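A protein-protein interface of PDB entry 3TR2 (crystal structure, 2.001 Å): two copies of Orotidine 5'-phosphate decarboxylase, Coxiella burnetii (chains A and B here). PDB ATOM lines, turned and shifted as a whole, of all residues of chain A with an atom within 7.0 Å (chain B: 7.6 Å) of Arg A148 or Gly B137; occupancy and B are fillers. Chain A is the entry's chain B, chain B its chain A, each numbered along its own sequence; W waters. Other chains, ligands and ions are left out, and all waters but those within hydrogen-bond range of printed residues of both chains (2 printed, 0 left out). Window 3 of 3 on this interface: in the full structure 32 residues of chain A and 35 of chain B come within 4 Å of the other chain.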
ATOM      1  N   ILE A  94     -24.310 -19.716 -30.785  1.00  0.00           N
ATOM      2  CA  ILE A  94     -23.208 -18.975 -30.183  1.00  0.00           C
ATOM      3  C   ILE A  94     -21.946 -19.845 -30.100  1.00  0.00           C
ATOM      4  O   ILE A  94     -20.829 -19.327 -30.091  1.00  0.00           O
ATOM      5  CB  ILE A  94     -23.593 -18.401 -28.803  1.00  0.00           C
ATOM      6  CG1 ILE A  94     -24.741 -17.384 -28.952  1.00  0.00           C
ATOM      7  CG2 ILE A  94     -22.370 -17.752 -28.134  1.00  0.00           C
ATOM      8  CD1 ILE A  94     -25.528 -17.103 -27.657  1.00  0.00           C
ATOM      9  N   GLY A 137     -16.805 -30.741 -22.934  1.00  0.00           N
ATOM     10  CA  GLY A 137     -15.827 -30.310 -21.954  1.00  0.00           C
ATOM     11  C   GLY A 137     -16.315 -29.176 -21.074  1.00  0.00           C
ATOM     12  O   GLY A 137     -15.515 -28.412 -20.533  1.00  0.00           O
ATOM     13  N   ILE A 138     -17.631 -29.066 -20.929  1.00  0.00           N
ATOM     14  CA  ILE A 138     -18.229 -28.037 -20.087  1.00  0.00           C
ATOM     15  C   ILE A 138     -18.385 -28.563 -18.664  1.00  0.00           C
ATOM     16  O   ILE A 138     -19.370 -29.224 -18.337  1.00  0.00           O
ATOM     17  CB  ILE A 138     -19.599 -27.588 -20.635  1.00  0.00           C
ATOM     18  CG1 ILE A 138     -19.467 -27.147 -22.092  1.00  0.00           C
ATOM     19  CG2 ILE A 138     -20.178 -26.462 -19.790  1.00  0.00           C
ATOM     20  CD1 ILE A 138     -20.774 -26.745 -22.736  1.00  0.00           C
ATOM     21  N   GLN A 139     -17.403 -28.276 -17.819  1.00  0.00           N
ATOM     22  CA  GLN A 139     -17.398 -28.823 -16.470  1.00  0.00           C
ATOM     23  C   GLN A 139     -18.389 -28.088 -15.579  1.00  0.00           C
ATOM     24  O   GLN A 139     -18.906 -28.654 -14.614  1.00  0.00           O
ATOM     25  CB  GLN A 139     -15.987 -28.787 -15.876  1.00  0.00           C
ATOM     26  CG  GLN A 139     -14.922 -29.393 -16.781  1.00  0.00           C
ATOM     27  CD  GLN A 139     -15.241 -30.817 -17.207  1.00  0.00           C
ATOM     28  OE1 GLN A 139     -16.048 -31.047 -18.111  1.00  0.00           O
ATOM     29  NE2 GLN A 139     -14.596 -31.786 -16.560  1.00  0.00           N
ATOM     30  N   GLU A 140     -18.657 -26.826 -15.906  1.00  0.00           N
ATOM     31  CA  GLU A 140     -19.658 -26.062 -15.173  1.00  0.00           C
ATOM     32  C   GLU A 140     -21.040 -26.399 -15.728  1.00  0.00           C
ATOM     33  O   GLU A 140     -21.165 -27.301 -16.558  1.00  0.00           O
ATOM     34  CB  GLU A 140     -19.374 -24.559 -15.232  1.00  0.00           C
ATOM     35  CG  GLU A 140     -19.634 -23.910 -16.575  1.00  0.00           C
ATOM     36  CD  GLU A 140     -19.446 -22.403 -16.531  1.00  0.00           C
ATOM     37  OE1 GLU A 140     -18.601 -21.928 -15.745  1.00  0.00           O
ATOM     38  OE2 GLU A 140     -20.152 -21.693 -17.279  1.00  0.00           O
ATOM     39  N   VAL A 142     -25.504 -25.509 -16.716  1.00  0.00           N
ATOM     40  CA  VAL A 142     -26.330 -24.754 -17.658  1.00  0.00           C
ATOM     41  C   VAL A 142     -26.490 -23.261 -17.344  1.00  0.00           C
ATOM     42  O   VAL A 142     -26.049 -22.422 -18.126  1.00  0.00           O
ATOM     43  CB  VAL A 142     -27.708 -25.431 -17.900  1.00  0.00           C
ATOM     44  CG1 VAL A 142     -28.547 -24.611 -18.867  1.00  0.00           C
ATOM     45  CG2 VAL A 142     -27.516 -26.847 -18.437  1.00  0.00           C
ATOM     46  N   PRO A 143     -27.105 -22.922 -16.199  1.00  0.00           N
ATOM     47  CA  PRO A 143     -27.335 -21.497 -15.935  1.00  0.00           C
ATOM     48  C   PRO A 143     -26.076 -20.667 -16.180  1.00  0.00           C
ATOM     49  O   PRO A 143     -26.158 -19.585 -16.766  1.00  0.00           O
ATOM     50  CB  PRO A 143     -27.714 -21.480 -14.452  1.00  0.00           C
ATOM     51  CG  PRO A 143     -28.327 -22.821 -14.218  1.00  0.00           C
ATOM     52  CD  PRO A 143     -27.536 -23.770 -15.073  1.00  0.00           C
ATOM     53  N   ASP A 144     -24.930 -21.188 -15.749  1.00  0.00           N
ATOM     54  CA  ASP A 144     -23.643 -20.512 -15.901  1.00  0.00           C
ATOM     55  C   ASP A 144     -23.229 -20.339 -17.361  1.00  0.00           C
ATOM     56  O   ASP A 144     -23.087 -19.216 -17.845  1.00  0.00           O
ATOM     57  CB  ASP A 144     -22.546 -21.284 -15.160  1.00  0.00           C
ATOM     58  CG  ASP A 144     -22.329 -20.784 -13.746  1.00  0.00           C
ATOM     59  OD1 ASP A 144     -23.162 -19.993 -13.253  1.00  0.00           O
ATOM     60  OD2 ASP A 144     -21.321 -21.192 -13.129  1.00  0.00           O
ATOM     61  N   ILE A 145     -23.017 -21.461 -18.043  1.00  0.00           N
ATOM     62  CA  ILE A 145     -22.561 -21.458 -19.432  1.00  0.00           C
ATOM     63  C   ILE A 145     -23.478 -20.628 -20.344  1.00  0.00           C
ATOM     64  O   ILE A 145     -23.008 -19.913 -21.224  1.00  0.00           O
ATOM     65  CB  ILE A 145     -22.403 -22.901 -19.967  1.00  0.00           C
ATOM     66  CG1 ILE A 145     -21.984 -22.900 -21.440  1.00  0.00           C
ATOM     67  CG2 ILE A 145     -23.677 -23.706 -19.739  1.00  0.00           C
ATOM     68  CD1 ILE A 145     -20.504 -22.658 -21.657  1.00  0.00           C
ATOM     69  N   VAL A 146     -24.782 -20.717 -20.112  1.00  0.00           N
ATOM     70  CA  VAL A 146     -25.746 -19.885 -20.824  1.00  0.00           C
ATOM     71  C   VAL A 146     -25.473 -18.395 -20.618  1.00  0.00           C
ATOM     72  O   VAL A 146     -25.473 -17.616 -21.571  1.00  0.00           O
ATOM     73  CB  VAL A 146     -27.185 -20.199 -20.387  1.00  0.00           C
ATOM     74  CG1 VAL A 146     -28.127 -19.095 -20.824  1.00  0.00           C
ATOM     75  CG2 VAL A 146     -27.622 -21.545 -20.946  1.00  0.00           C
ATOM     76  N   CYS A 147     -25.233 -17.998 -19.371  1.00  0.00           N
ATOM     77  CA  CYS A 147     -24.970 -16.594 -19.082  1.00  0.00           C
ATOM     78  C   CYS A 147     -23.663 -16.159 -19.744  1.00  0.00           C
ATOM     79  O   CYS A 147     -23.512 -15.008 -20.155  1.00  0.00           O
ATOM     80  CB  CYS A 147     -24.922 -16.339 -17.571  1.00  0.00           C
ATOM     81  SG  CYS A 147     -24.822 -14.585 -17.140  1.00  0.00           S
ATOM     82  N   ARG A 148     -22.725 -17.091 -19.851  1.00  0.00           N
ATOM     83  CA  ARG A 148     -21.442 -16.819 -20.481  1.00  0.00           C
ATOM     84  C   ARG A 148     -21.592 -16.616 -21.990  1.00  0.00           C
ATOM     85  O   ARG A 148     -21.015 -15.694 -22.567  1.00  0.00           O
ATOM     86  CB  ARG A 148     -20.469 -17.965 -20.206  1.00  0.00           C
ATOM     87  CG  ARG A 148     -19.011 -17.585 -20.368  1.00  0.00           C
ATOM     88  CD  ARG A 148     -18.124 -18.817 -20.382  1.00  0.00           C
ATOM     89  NE  ARG A 148     -17.780 -19.282 -19.045  1.00  0.00           N
ATOM     90  CZ  ARG A 148     -16.619 -19.029 -18.446  1.00  0.00           C
ATOM     91  NH1 ARG A 148     -15.691 -18.312 -19.063  1.00  0.00           N
ATOM     92  NH2 ARG A 148     -16.389 -19.498 -17.230  1.00  0.00           N
ATOM     93  N   MET A 149     -22.360 -17.492 -22.629  1.00  0.00           N
ATOM     94  CA  MET A 149     -22.590 -17.397 -24.062  1.00  0.00           C
ATOM     95  C   MET A 149     -23.409 -16.155 -24.384  1.00  0.00           C
ATOM     96  O   MET A 149     -23.205 -15.515 -25.419  1.00  0.00           O
ATOM     97  CB  MET A 149     -23.302 -18.652 -24.581  1.00  0.00           C
ATOM     98  CG  MET A 149     -22.593 -19.932 -24.218  1.00  0.00           C
ATOM     99  SD  MET A 149     -23.387 -21.510 -25.003  1.00  0.00           S
ATOM    100  CE  MET A 149     -22.765 -21.315 -26.822  1.00  0.00           C
ATOM    101  N   ALA A 150     -24.340 -15.819 -23.495  1.00  0.00           N
ATOM    102  CA  ALA A 150     -25.212 -14.672 -23.720  1.00  0.00           C
ATOM    103  C   ALA A 150     -24.393 -13.392 -23.761  1.00  0.00           C
ATOM    104  O   ALA A 150     -24.653 -12.494 -24.562  1.00  0.00           O
ATOM    105  CB  ALA A 150     -26.279 -14.588 -22.642  1.00  0.00           C
ATOM    106  N   THR A 151     -23.404 -13.322 -22.881  1.00  0.00           N
ATOM    107  CA  THR A 151     -22.521 -12.174 -22.779  1.00  0.00           C
ATOM    108  C   THR A 151     -21.699 -12.024 -24.049  1.00  0.00           C
ATOM    109  O   THR A 151     -21.596 -10.929 -24.608  1.00  0.00           O
ATOM    110  CB  THR A 151     -21.588 -12.333 -21.570  1.00  0.00           C
ATOM    111  OG1 THR A 151     -22.382 -12.518 -20.392  1.00  0.00           O
ATOM    112  CG2 THR A 151     -20.705 -11.105 -21.402  1.00  0.00           C
ATOM    113  N   LEU A 152     -21.130 -13.141 -24.502  1.00  0.00           N
ATOM    114  CA  LEU A 152     -20.401 -13.187 -25.760  1.00  0.00           C
ATOM    115  C   LEU A 152     -21.296 -12.718 -26.909  1.00  0.00           C
ATOM    116  O   LEU A 152     -20.900 -11.866 -27.706  1.00  0.00           O
ATOM    117  CB  LEU A 152     -19.900 -14.611 -26.032  1.00  0.00           C
ATOM    118  CG  LEU A 152     -18.979 -14.787 -27.243  1.00  0.00           C
ATOM    119  CD1 LEU A 152     -17.701 -13.976 -27.054  1.00  0.00           C
ATOM    120  CD2 LEU A 152     -18.649 -16.253 -27.494  1.00  0.00           C
ATOM    121  N   ALA A 153     -22.505 -13.266 -26.984  1.00  0.00           N
ATOM    122  CA  ALA A 153     -23.427 -12.889 -28.056  1.00  0.00           C
ATOM    123  C   ALA A 153     -23.625 -11.378 -28.080  1.00  0.00           C
ATOM    124  O   ALA A 153     -23.590 -10.759 -29.141  1.00  0.00           O
ATOM    125  CB  ALA A 153     -24.766 -13.603 -27.899  1.00  0.00           C
ATOM    126  N   LEU A 171     -31.041 -13.525 -16.970  1.00  0.00           N
ATOM    127  CA  LEU A 171     -30.368 -12.783 -18.031  1.00  0.00           C
ATOM    128  C   LEU A 171     -30.808 -11.326 -18.063  1.00  0.00           C
ATOM    129  O   LEU A 171     -30.031 -10.437 -18.407  1.00  0.00           O
ATOM    130  CB  LEU A 171     -30.619 -13.432 -19.393  1.00  0.00           C
ATOM    131  CG  LEU A 171     -30.068 -14.842 -19.580  1.00  0.00           C
ATOM    132  CD1 LEU A 171     -30.484 -15.384 -20.941  1.00  0.00           C
ATOM    133  CD2 LEU A 171     -28.560 -14.837 -19.448  1.00  0.00           C
ATOM    134  N   PHE A 175     -28.731  -8.163 -18.567  1.00  0.00           N
ATOM    135  CA  PHE A 175     -28.943  -7.295 -19.723  1.00  0.00           C
ATOM    136  C   PHE A 175     -30.231  -6.504 -19.585  1.00  0.00           C
ATOM    137  O   PHE A 175     -31.316  -7.074 -19.444  1.00  0.00           O
ATOM    138  CB  PHE A 175     -28.972  -8.112 -21.014  1.00  0.00           C
ATOM    139  CG  PHE A 175     -27.779  -8.989 -21.194  1.00  0.00           C
ATOM    140  CD1 PHE A 175     -26.604  -8.477 -21.711  1.00  0.00           C
ATOM    141  CD2 PHE A 175     -27.828 -10.326 -20.843  1.00  0.00           C
ATOM    142  CE1 PHE A 175     -25.496  -9.283 -21.876  1.00  0.00           C
ATOM    143  CE2 PHE A 175     -26.723 -11.139 -21.006  1.00  0.00           C
ATOM    144  CZ  PHE A 175     -25.556 -10.616 -21.523  1.00  0.00           C
ATOM    145  N   SER B 131      -8.649 -21.151 -28.111  1.00  0.00           N
ATOM    146  CA  SER B 131      -8.979 -19.817 -27.629  1.00  0.00           C
ATOM    147  C   SER B 131     -10.497 -19.634 -27.557  1.00  0.00           C
ATOM    148  O   SER B 131     -11.011 -19.014 -26.634  1.00  0.00           O
ATOM    149  CB  SER B 131      -8.320 -18.732 -28.491  1.00  0.00           C
ATOM    150  OG  SER B 131      -8.963 -18.594 -29.742  1.00  0.00           O
ATOM    151  N   ASP B 132     -11.219 -20.200 -28.520  1.00  0.00           N
ATOM    152  CA  ASP B 132     -12.677 -20.150 -28.491  1.00  0.00           C
ATOM    153  C   ASP B 132     -13.206 -20.986 -27.335  1.00  0.00           C
ATOM    154  O   ASP B 132     -14.108 -20.561 -26.604  1.00  0.00           O
ATOM    155  CB  ASP B 132     -13.267 -20.656 -29.817  1.00  0.00           C
ATOM    156  CG  ASP B 132     -12.820 -19.829 -31.001  1.00  0.00           C
ATOM    157  OD1 ASP B 132     -13.274 -18.676 -31.125  1.00  0.00           O
ATOM    158  OD2 ASP B 132     -12.020 -20.326 -31.817  1.00  0.00           O
ATOM    159  N   LEU B 133     -12.638 -22.175 -27.167  1.00  0.00           N
ATOM    160  CA  LEU B 133     -13.076 -23.077 -26.106  1.00  0.00           C
ATOM    161  C   LEU B 133     -12.919 -22.450 -24.725  1.00  0.00           C
ATOM    162  O   LEU B 133     -13.806 -22.569 -23.881  1.00  0.00           O
ATOM    163  CB  LEU B 133     -12.316 -24.403 -26.166  1.00  0.00           C
ATOM    164  CG  LEU B 133     -12.662 -25.326 -27.332  1.00  0.00           C
ATOM    165  CD1 LEU B 133     -11.790 -26.571 -27.288  1.00  0.00           C
ATOM    166  CD2 LEU B 133     -14.134 -25.699 -27.301  1.00  0.00           C
ATOM    167  N   LYS B 134     -11.791 -21.784 -24.495  1.00  0.00           N
ATOM    168  CA  LYS B 134     -11.519 -21.206 -23.185  1.00  0.00           C
ATOM    169  C   LYS B 134     -12.469 -20.052 -22.877  1.00  0.00           C
ATOM    170  O   LYS B 134     -12.798 -19.796 -21.720  1.00  0.00           O
ATOM    171  CB  LYS B 134     -10.060 -20.752 -23.081  1.00  0.00           C
ATOM    172  CG  LYS B 134      -9.062 -21.896 -23.169  1.00  0.00           C
ATOM    173  CD  LYS B 134      -7.623 -21.408 -23.043  1.00  0.00           C
ATOM    174  CE  LYS B 134      -6.650 -22.457 -23.571  1.00  0.00           C
ATOM    175  NZ  LYS B 134      -6.805 -23.766 -22.878  1.00  0.00           N
ATOM    176  N   THR B 135     -12.915 -19.359 -23.919  1.00  0.00           N
ATOM    177  CA  THR B 135     -13.862 -18.268 -23.738  1.00  0.00           C
ATOM    178  C   THR B 135     -15.155 -18.807 -23.132  1.00  0.00           C
ATOM    179  O   THR B 135     -15.878 -18.086 -22.451  1.00  0.00           O
ATOM    180  CB  THR B 135     -14.127 -17.518 -25.056  1.00  0.00           C
ATOM    181  OG1 THR B 135     -12.977 -16.724 -25.378  1.00  0.00           O
ATOM    182  CG2 THR B 135     -15.337 -16.605 -24.929  1.00  0.00           C
ATOM    183  N   LEU B 136     -15.421 -20.090 -23.362  1.00  0.00           N
ATOM    184  CA  LEU B 136     -16.583 -20.752 -22.781  1.00  0.00           C
ATOM    185  C   LEU B 136     -16.222 -21.524 -21.508  1.00  0.00           C
ATOM    186  O   LEU B 136     -17.022 -22.310 -21.004  1.00  0.00           O
ATOM    187  CB  LEU B 136     -17.229 -21.688 -23.807  1.00  0.00           C
ATOM    188  CG  LEU B 136     -17.535 -21.022 -25.153  1.00  0.00           C
ATOM    189  CD1 LEU B 136     -18.111 -22.012 -26.156  1.00  0.00           C
ATOM    190  CD2 LEU B 136     -18.467 -19.830 -24.961  1.00  0.00           C
ATOM    191  N   GLY B 137     -15.020 -21.295 -20.990  1.00  0.00           N
ATOM    192  CA  GLY B 137     -14.561 -21.986 -19.797  1.00  0.00           C
ATOM    193  C   GLY B 137     -14.134 -23.423 -20.055  1.00  0.00           C
ATOM    194  O   GLY B 137     -13.940 -24.195 -19.119  1.00  0.00           O
ATOM    195  N   ILE B 138     -13.988 -23.784 -21.326  1.00  0.00           N
ATOM    196  CA  ILE B 138     -13.523 -25.117 -21.693  1.00  0.00           C
ATOM    197  C   ILE B 138     -12.001 -25.143 -21.714  1.00  0.00           C
ATOM    198  O   ILE B 138     -11.377 -24.430 -22.493  1.00  0.00           O
ATOM    199  CB  ILE B 138     -14.032 -25.542 -23.086  1.00  0.00           C
ATOM    200  CG1 ILE B 138     -15.536 -25.289 -23.212  1.00  0.00           C
ATOM    201  CG2 ILE B 138     -13.692 -27.003 -23.365  1.00  0.00           C
ATOM    202  CD1 ILE B 138     -16.332 -25.846 -22.071  1.00  0.00           C
ATOM    203  N   GLN B 139     -11.407 -25.970 -20.862  1.00  0.00           N
ATOM    204  CA  GLN B 139      -9.950 -26.027 -20.756  1.00  0.00           C
ATOM    205  C   GLN B 139      -9.354 -27.217 -21.503  1.00  0.00           C
ATOM    206  O   GLN B 139      -8.157 -27.246 -21.781  1.00  0.00           O
ATOM    207  CB  GLN B 139      -9.523 -26.051 -19.287  1.00  0.00           C
ATOM    208  CG  GLN B 139      -9.966 -24.825 -18.501  1.00  0.00           C
ATOM    209  CD  GLN B 139      -9.348 -23.543 -19.028  1.00  0.00           C
ATOM    210  OE1 GLN B 139      -8.216 -23.538 -19.516  1.00  0.00           O
ATOM    211  NE2 GLN B 139     -10.091 -22.447 -18.935  1.00  0.00           N
ATOM    212  N   GLU B 140     -10.193 -28.193 -21.835  1.00  0.00           N
ATOM    213  CA  GLU B 140      -9.727 -29.378 -22.547  1.00  0.00           C
ATOM    214  C   GLU B 140      -9.243 -29.025 -23.955  1.00  0.00           C
ATOM    215  O   GLU B 140      -9.682 -28.033 -24.538  1.00  0.00           O
ATOM    216  CB  GLU B 140     -10.822 -30.444 -22.592  1.00  0.00           C
ATOM    217  CG  GLU B 140     -11.179 -30.996 -21.225  1.00  0.00           C
ATOM    218  CD  GLU B 140     -12.288 -32.022 -21.283  1.00  0.00           C
ATOM    219  OE1 GLU B 140     -12.653 -32.429 -22.403  1.00  0.00           O
ATOM    220  OE2 GLU B 140     -12.799 -32.418 -20.213  1.00  0.00           O
HETATM  221  O   HOH W   1     -15.094 -33.418 -20.181  1.00  0.00           O
HETATM  222  O   HOH W   2     -12.799 -27.799 -19.474  1.00  0.00           O
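O of Thr B135 sits close to NH1 of Arg A148, 3.4 Å away.
The backbone carbonyl oxygen (O) of Ser B131 sits at hydrogen-bond distance from the side-chain hydroxyl (OG1) of Thr B135 (3.3 Å).
O of Leu B133 sits at hydrogen-bond distance from N of Ile B138 (2.8 Å).
OE2 of Glu A140 lies within hydrogen-bond range of N of Ile A145, at 3.0 Å.
The side-chain carboxylate (OE1) of Glu A140 lies within salt-bridge range of the guanidinium group (NH2) of Arg A148 (3.6 Å).
Among the printed residues, merely in contact across the chains: Gly A137 with Ile B138 (3.1 Å), Ile A138 with Ile B138 (3.4 Å), Arg A148 with Leu B136 (3.4 Å), Ile A145 with Leu B136 (3.6 Å), Arg A148 with Gly B137 (3.6 Å) and Gly A137 with Glu B140 (3.8 Å).
Arg A148 touches just these residues of chain B: Thr B135 (3.1 Å), Leu B136 (3.4 Å) and Gly B137 (3.6 Å).
Gly B137 touches just one residue of chain A: Arg A148 (3.6 Å).
Printed residues of chain B within 4 Å of Ile A145: Leu B136 (3.6 Å).
Printed residues of chain B within 4 Å of Gly A137: Ile B138 and Glu B140.
Asp A144 touches none of the printed residues of chain B.
Cys A147 touches none of the printed residues of chain B.
Of the 10 printed residues of chain B, 5 touch a printed residue of chain A.
Hydrophobic or aromatic side chains of chain B that line the printed part of chain A: Ile B138.
Along chain B the printed residues that touch a printed residue of chain A span positions 135 to 140.
Of the 19 printed residues of chain A, 4 touch a printed residue of chain B.
Hydrophobic or aromatic side chains of chain A that line the printed part of chain B: Ile A138 and Ile A145.
Among the printed residues, no Asp or Glu carboxylate lies within 4 Å of a Lys or Arg side-chain nitrogen of the other chain.
Gly A137 touches Ile B138, but with the chains exchanged Ile A138 does not touch Gly B137 (5.8 Å).
Gly A137 touches Glu B140, but with the chains exchanged Glu A140 does not touch Gly B137 (5.7 Å).
Ile A138 touches its own counterpart, Ile B138.
Of the 7 pairs that touch across the chains among the printed residues, 1 has its exchanged pair printed and touching as well.
Water W1 lies within hydrogen-bond range of OE2 of Glu B140 (2.5 Å) and OE1 of Gln A139 (3.3 Å).
Water W2 lies within hydrogen-bond range of the backbone NH (N) of Gln B139 (2.7 Å) and the backbone carbonyl oxygen (O) of Gly A137 (3.0 Å).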
